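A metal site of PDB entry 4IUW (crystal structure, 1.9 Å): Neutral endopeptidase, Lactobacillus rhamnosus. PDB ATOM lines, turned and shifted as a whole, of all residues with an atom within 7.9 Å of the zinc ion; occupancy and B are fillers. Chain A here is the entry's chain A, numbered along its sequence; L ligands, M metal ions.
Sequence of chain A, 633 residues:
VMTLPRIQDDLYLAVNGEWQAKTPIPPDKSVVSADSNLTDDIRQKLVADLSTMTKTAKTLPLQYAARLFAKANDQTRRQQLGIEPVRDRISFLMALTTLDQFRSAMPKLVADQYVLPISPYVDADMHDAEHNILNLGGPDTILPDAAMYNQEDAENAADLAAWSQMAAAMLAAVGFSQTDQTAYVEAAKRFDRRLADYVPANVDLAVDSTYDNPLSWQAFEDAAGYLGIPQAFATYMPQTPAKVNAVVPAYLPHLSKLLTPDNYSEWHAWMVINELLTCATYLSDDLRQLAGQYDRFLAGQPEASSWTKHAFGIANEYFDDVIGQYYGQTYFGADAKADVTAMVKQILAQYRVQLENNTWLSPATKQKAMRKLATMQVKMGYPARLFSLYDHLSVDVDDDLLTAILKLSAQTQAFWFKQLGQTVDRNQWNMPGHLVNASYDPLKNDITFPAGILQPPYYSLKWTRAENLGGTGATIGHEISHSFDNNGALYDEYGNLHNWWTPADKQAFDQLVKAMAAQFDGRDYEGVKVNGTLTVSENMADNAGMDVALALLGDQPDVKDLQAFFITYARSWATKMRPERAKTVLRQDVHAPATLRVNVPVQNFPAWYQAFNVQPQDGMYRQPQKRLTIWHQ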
ATOM      1  N   ASN A 437      18.530  -9.352 -24.129  1.00  0.00           N
ATOM      2  CA  ASN A 437      17.788  -8.423 -23.322  1.00  0.00           C
ATOM      3  C   ASN A 437      16.532  -9.149 -22.833  1.00  0.00           C
ATOM      4  O   ASN A 437      16.312 -10.305 -23.192  1.00  0.00           O
ATOM      5  CB  ASN A 437      17.411  -7.195 -24.132  1.00  0.00           C
ATOM      6  CG  ASN A 437      17.325  -5.928 -23.275  1.00  0.00           C
ATOM      7  OD1 ASN A 437      16.968  -5.951 -22.101  1.00  0.00           O
ATOM      8  ND2 ASN A 437      17.641  -4.792 -23.909  1.00  0.00           N
ATOM      9  N   ALA A 438      15.682  -8.421 -22.095  1.00  0.00           N
ATOM     10  CA  ALA A 438      14.422  -8.990 -21.587  1.00  0.00           C
ATOM     11  C   ALA A 438      13.546  -7.787 -21.195  1.00  0.00           C
ATOM     12  O   ALA A 438      14.053  -6.654 -21.058  1.00  0.00           O
ATOM     13  CB  ALA A 438      14.677  -9.874 -20.357  1.00  0.00           C
ATOM     14  N   SER A 439      12.264  -8.040 -21.015  1.00  0.00           N
ATOM     15  CA  SER A 439      11.297  -6.950 -20.827  1.00  0.00           C
ATOM     16  C   SER A 439      10.017  -7.301 -20.095  1.00  0.00           C
ATOM     17  O   SER A 439       9.595  -8.450 -19.997  1.00  0.00           O
ATOM     18  CB  SER A 439      10.889  -6.400 -22.147  1.00  0.00           C
ATOM     19  OG  SER A 439      10.158  -7.374 -22.866  1.00  0.00           O
ATOM     20  N   TYR A 440       9.346  -6.234 -19.712  1.00  0.00           N
ATOM     21  CA  TYR A 440       8.035  -6.200 -19.087  1.00  0.00           C
ATOM     22  C   TYR A 440       7.257  -5.066 -19.782  1.00  0.00           C
ATOM     23  O   TYR A 440       7.807  -3.946 -19.993  1.00  0.00           O
ATOM     24  CB  TYR A 440       8.089  -5.868 -17.609  1.00  0.00           C
ATOM     25  CG  TYR A 440       6.699  -5.620 -17.032  1.00  0.00           C
ATOM     26  CD1 TYR A 440       5.853  -6.697 -16.738  1.00  0.00           C
ATOM     27  CD2 TYR A 440       6.177  -4.321 -16.866  1.00  0.00           C
ATOM     28  CE1 TYR A 440       4.582  -6.494 -16.262  1.00  0.00           C
ATOM     29  CE2 TYR A 440       4.900  -4.128 -16.431  1.00  0.00           C
ATOM     30  CZ  TYR A 440       4.107  -5.224 -16.126  1.00  0.00           C
ATOM     31  OH  TYR A 440       2.831  -5.052 -15.645  1.00  0.00           O
ATOM     32  N   THR A 475      17.086 -11.672 -13.214  1.00  0.00           N
ATOM     33  CA  THR A 475      16.433 -11.091 -14.383  1.00  0.00           C
ATOM     34  C   THR A 475      14.937 -11.392 -14.530  1.00  0.00           C
ATOM     35  O   THR A 475      14.118 -10.473 -14.728  1.00  0.00           O
ATOM     36  CB  THR A 475      17.175 -11.458 -15.674  1.00  0.00           C
ATOM     37  OG1 THR A 475      18.529 -11.000 -15.604  1.00  0.00           O
ATOM     38  CG2 THR A 475      16.501 -10.779 -16.872  1.00  0.00           C
ATOM     39  N   HIS A 478      13.359  -9.424 -11.876  1.00  0.00           N
ATOM     40  CA  HIS A 478      13.397  -8.051 -12.266  1.00  0.00           C
ATOM     41  C   HIS A 478      12.200  -7.727 -13.167  1.00  0.00           C
ATOM     42  O   HIS A 478      11.495  -6.737 -12.935  1.00  0.00           O
ATOM     43  CB  HIS A 478      14.733  -7.775 -13.009  1.00  0.00           C
ATOM     44  CG  HIS A 478      14.869  -6.390 -13.568  1.00  0.00           C
ATOM     45  ND1 HIS A 478      15.749  -5.476 -13.040  1.00  0.00           N
ATOM     46  CD2 HIS A 478      14.311  -5.793 -14.655  1.00  0.00           C
ATOM     47  CE1 HIS A 478      15.699  -4.348 -13.738  1.00  0.00           C
ATOM     48  NE2 HIS A 478      14.830  -4.502 -14.711  1.00  0.00           N
ATOM     49  N   GLU A 479      11.991  -8.550 -14.188  1.00  0.00           N
ATOM     50  CA  GLU A 479      10.933  -8.274 -15.126  1.00  0.00           C
ATOM     51  C   GLU A 479       9.563  -8.335 -14.427  1.00  0.00           C
ATOM     52  O   GLU A 479       8.678  -7.453 -14.638  1.00  0.00           O
ATOM     53  CB  GLU A 479      11.021  -9.194 -16.359  1.00  0.00           C
ATOM     54  CG  GLU A 479      12.253  -9.064 -17.260  1.00  0.00           C
ATOM     55  CD  GLU A 479      12.673  -7.660 -17.652  1.00  0.00           C
ATOM     56  OE1 GLU A 479      11.860  -6.701 -17.597  1.00  0.00           O
ATOM     57  OE2 GLU A 479      13.904  -7.520 -17.946  1.00  0.00           O
ATOM     58  N   SER A 481       9.009  -7.726 -11.323  1.00  0.00           N
ATOM     59  CA  SER A 481       8.977  -6.534 -10.454  1.00  0.00           C
ATOM     60  C   SER A 481       8.585  -5.233 -11.125  1.00  0.00           C
ATOM     61  O   SER A 481       8.081  -4.296 -10.414  1.00  0.00           O
ATOM     62  CB  SER A 481      10.299  -6.368  -9.708  1.00  0.00           C
ATOM     63  OG  SER A 481      10.585  -7.554  -8.976  1.00  0.00           O
ATOM     64  N   HIS A 482       8.828  -5.138 -12.429  1.00  0.00           N
ATOM     65  CA  HIS A 482       8.356  -4.006 -13.173  1.00  0.00           C
ATOM     66  C   HIS A 482       6.825  -3.825 -13.173  1.00  0.00           C
ATOM     67  O   HIS A 482       6.370  -2.694 -13.348  1.00  0.00           O
ATOM     68  CB  HIS A 482       8.822  -4.055 -14.587  1.00  0.00           C
ATOM     69  CG  HIS A 482      10.121  -3.379 -14.818  1.00  0.00           C
ATOM     70  ND1 HIS A 482      10.419  -2.154 -14.300  1.00  0.00           N
ATOM     71  CD2 HIS A 482      11.202  -3.763 -15.528  1.00  0.00           C
ATOM     72  CE1 HIS A 482      11.643  -1.793 -14.689  1.00  0.00           C
ATOM     73  NE2 HIS A 482      12.109  -2.744 -15.472  1.00  0.00           N
ATOM     74  N   ASP A 485       6.635  -1.543 -10.093  1.00  0.00           N
ATOM     75  CA  ASP A 485       7.542  -0.444  -9.861  1.00  0.00           C
ATOM     76  C   ASP A 485       6.728   0.888  -9.848  1.00  0.00           C
ATOM     77  O   ASP A 485       5.495   0.878  -9.738  1.00  0.00           O
ATOM     78  CB  ASP A 485       8.768  -0.467 -10.778  1.00  0.00           C
ATOM     79  CG  ASP A 485       8.460  -0.038 -12.238  1.00  0.00           C
ATOM     80  OD1 ASP A 485       7.406   0.584 -12.570  1.00  0.00           O
ATOM     81  OD2 ASP A 485       9.367  -0.242 -13.070  1.00  0.00           O
ATOM     82  N   SER A 537      13.029   3.371 -11.058  1.00  0.00           N
ATOM     83  CA  SER A 537      12.209   2.246 -11.531  1.00  0.00           C
ATOM     84  C   SER A 537      13.010   0.939 -11.694  1.00  0.00           C
ATOM     85  O   SER A 537      12.554  -0.170 -11.302  1.00  0.00           O
ATOM     86  CB  SER A 537      11.553   2.595 -12.823  1.00  0.00           C
ATOM     87  OG  SER A 537      12.527   2.932 -13.823  1.00  0.00           O
ATOM     88  N   GLU A 538      14.205   1.094 -12.268  1.00  0.00           N
ATOM     89  CA  GLU A 538      15.103  -0.030 -12.481  1.00  0.00           C
ATOM     90  C   GLU A 538      15.794  -0.533 -11.246  1.00  0.00           C
ATOM     91  O   GLU A 538      16.079  -1.735 -11.154  1.00  0.00           O
ATOM     92  CB  GLU A 538      16.159   0.330 -13.540  1.00  0.00           C
ATOM     93  CG  GLU A 538      15.544   0.654 -14.921  1.00  0.00           C
ATOM     94  CD  GLU A 538      14.790  -0.470 -15.519  1.00  0.00           C
ATOM     95  OE1 GLU A 538      15.171  -1.637 -15.222  1.00  0.00           O
ATOM     96  OE2 GLU A 538      13.915  -0.181 -16.398  1.00  0.00           O
ATOM     97  N   ASN A 539      16.124   0.376 -10.333  1.00  0.00           N
ATOM     98  CA  ASN A 539      16.702  -0.004  -9.063  1.00  0.00           C
ATOM     99  C   ASN A 539      15.671  -0.699  -8.172  1.00  0.00           C
ATOM    100  O   ASN A 539      15.997  -1.644  -7.470  1.00  0.00           O
ATOM    101  CB  ASN A 539      17.341   1.161  -8.352  1.00  0.00           C
ATOM    102  CG  ASN A 539      18.529   1.706  -9.129  1.00  0.00           C
ATOM    103  OD1 ASN A 539      19.280   0.962  -9.731  1.00  0.00           O
ATOM    104  ND2 ASN A 539      18.747   2.980  -9.044  1.00  0.00           N
ATOM    105  N   ALA A 541      13.197  -2.622  -9.505  1.00  0.00           N
ATOM    106  CA  ALA A 541      13.117  -3.921 -10.129  1.00  0.00           C
ATOM    107  C   ALA A 541      14.293  -4.823  -9.806  1.00  0.00           C
ATOM    108  O   ALA A 541      14.137  -6.059  -9.661  1.00  0.00           O
ATOM    109  CB  ALA A 541      12.942  -3.783 -11.621  1.00  0.00           C
ATOM    110  N   ASP A 542      15.481  -4.229  -9.769  1.00  0.00           N
ATOM    111  CA  ASP A 542      16.687  -5.007  -9.400  1.00  0.00           C
ATOM    112  C   ASP A 542      16.585  -5.537  -8.012  1.00  0.00           C
ATOM    113  O   ASP A 542      17.076  -6.653  -7.740  1.00  0.00           O
ATOM    114  CB  ASP A 542      17.948  -4.116  -9.458  1.00  0.00           C
ATOM    115  CG  ASP A 542      18.461  -3.950 -10.868  1.00  0.00           C
ATOM    116  OD1 ASP A 542      18.071  -4.707 -11.796  1.00  0.00           O
ATOM    117  OD2 ASP A 542      19.320  -3.067 -11.035  1.00  0.00           O
ATOM    118  N   TRP A 573      27.120  -8.986 -15.310  1.00  0.00           N
ATOM    119  CA  TRP A 573      27.016  -7.558 -15.450  1.00  0.00           C
ATOM    120  C   TRP A 573      28.340  -6.865 -15.844  1.00  0.00           C
ATOM    121  O   TRP A 573      28.437  -5.642 -15.802  1.00  0.00           O
ATOM    122  CB  TRP A 573      26.494  -6.932 -14.144  1.00  0.00           C
ATOM    123  CG  TRP A 573      25.012  -7.006 -14.002  1.00  0.00           C
ATOM    124  CD1 TRP A 573      24.309  -7.742 -13.101  1.00  0.00           C
ATOM    125  CD2 TRP A 573      24.041  -6.370 -14.870  1.00  0.00           C
ATOM    126  NE1 TRP A 573      22.938  -7.592 -13.347  1.00  0.00           N
ATOM    127  CE2 TRP A 573      22.767  -6.756 -14.422  1.00  0.00           C
ATOM    128  CE3 TRP A 573      24.145  -5.534 -15.992  1.00  0.00           C
ATOM    129  CZ2 TRP A 573      21.563  -6.297 -15.039  1.00  0.00           C
ATOM    130  CZ3 TRP A 573      22.933  -5.050 -16.582  1.00  0.00           C
ATOM    131  CH2 TRP A 573      21.683  -5.476 -16.101  1.00  0.00           C
ATOM    132  N   VAL A 590      17.200   5.082 -17.698  1.00  0.00           N
ATOM    133  CA  VAL A 590      16.602   4.695 -16.440  1.00  0.00           C
ATOM    134  C   VAL A 590      17.372   3.602 -15.665  1.00  0.00           C
ATOM    135  O   VAL A 590      17.098   3.362 -14.491  1.00  0.00           O
ATOM    136  CB  VAL A 590      15.129   4.269 -16.630  1.00  0.00           C
ATOM    137  CG1 VAL A 590      14.315   5.496 -17.105  1.00  0.00           C
ATOM    138  CG2 VAL A 590      14.964   3.123 -17.642  1.00  0.00           C
ATOM    139  N   HIS A 591      18.319   2.932 -16.307  1.00  0.00           N
ATOM    140  CA  HIS A 591      19.157   1.978 -15.607  1.00  0.00           C
ATOM    141  C   HIS A 591      20.346   2.608 -14.975  1.00  0.00           C
ATOM    142  O   HIS A 591      21.035   3.416 -15.607  1.00  0.00           O
ATOM    143  CB  HIS A 591      19.647   0.902 -16.566  1.00  0.00           C
ATOM    144  CG  HIS A 591      18.570   0.236 -17.324  1.00  0.00           C
ATOM    145  ND1 HIS A 591      18.158   0.634 -18.591  1.00  0.00           N
ATOM    146  CD2 HIS A 591      17.816  -0.854 -17.003  1.00  0.00           C
ATOM    147  CE1 HIS A 591      17.144  -0.139 -18.963  1.00  0.00           C
ATOM    148  NE2 HIS A 591      16.939  -1.058 -18.031  1.00  0.00           N
ATOM    149  N   ARG A 597      24.646  -1.584 -10.086  1.00  0.00           N
ATOM    150  CA  ARG A 597      23.589  -2.623 -10.127  1.00  0.00           C
ATOM    151  C   ARG A 597      24.091  -3.910  -9.487  1.00  0.00           C
ATOM    152  O   ARG A 597      23.300  -4.738  -9.053  1.00  0.00           O
ATOM    153  CB  ARG A 597      23.104  -2.895 -11.519  1.00  0.00           C
ATOM    154  CG  ARG A 597      22.457  -1.652 -12.146  1.00  0.00           C
ATOM    155  CD  ARG A 597      21.978  -1.985 -13.547  1.00  0.00           C
ATOM    156  NE  ARG A 597      20.753  -2.766 -13.512  1.00  0.00           N
ATOM    157  CZ  ARG A 597      20.021  -3.014 -14.593  1.00  0.00           C
ATOM    158  NH1 ARG A 597      20.407  -2.601 -15.795  1.00  0.00           N
ATOM    159  NH2 ARG A 597      18.895  -3.665 -14.474  1.00  0.00           N
HETATM  160  C1  LIG L   1      18.354  -7.519 -18.515  1.00  0.00           C
HETATM  161  O1  LIG L   1      19.234  -7.362 -17.644  1.00  0.00           O
HETATM  162  O2  LIG L   1      18.560  -8.428 -19.302  1.00  0.00           O
HETATM  163  C2  LIG L   1      17.047  -6.685 -18.674  1.00  0.00           C
HETATM  164  C3  LIG L   1      17.326  -5.191 -18.966  1.00  0.00           C
HETATM  165  O3  LIG L   1      18.337  -4.989 -19.963  1.00  0.00           O
HETATM  166  C4  LIG L   1      16.043  -4.451 -19.414  1.00  0.00           C
HETATM  167  C5  LIG L   1      15.037  -4.207 -18.294  1.00  0.00           C
HETATM  168  O4  LIG L   1      14.915  -3.018 -17.852  1.00  0.00           O
HETATM  169  O5  LIG L   1      14.328  -5.203 -17.896  1.00  0.00           O
HETATM  170  C6  LIG L   1      17.960  -4.509 -17.772  1.00  0.00           C
HETATM  171  O6  LIG L   1      18.992  -3.811 -17.981  1.00  0.00           O
HETATM  172  O7  LIG L   1      17.439  -4.623 -16.612  1.00  0.00           O
HETATM  173 ZN    ZN M   1      14.208  -3.109 -16.071  1.00  0.00          ZN
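Residues that only touch the zinc ion: His 591. Four residues have an atom within 4 Å of the zinc ion: His 478, His 482, Glu 538 and His 591. Along chain A the residues within 4 Å of the zinc ion span positions 478 to 591.
The side-chain carboxylate (OD2) of Asp 485 lies within hydrogen-bond range of a ring nitrogen (ND1) of His 482 (2.5 Å). OE1 of Glu 538 sits close to NE2 of His 591 (3.4 Å). A ring nitrogen (ND1) of His 478 is in hydrogen-bond range of the side-chain carboxylate (OD1) of Asp 542, 2.7 Å away.
The zinc ion is bound by an oxygen (O4) of the ligand, the side-chain carboxylate of Glu 538, a ring nitrogen (NE2) of His 478 and a ring nitrogen (NE2) of His 482. Slightly farther from the zinc ion lies an oxygen (O5) of the ligand (2.8 Å).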
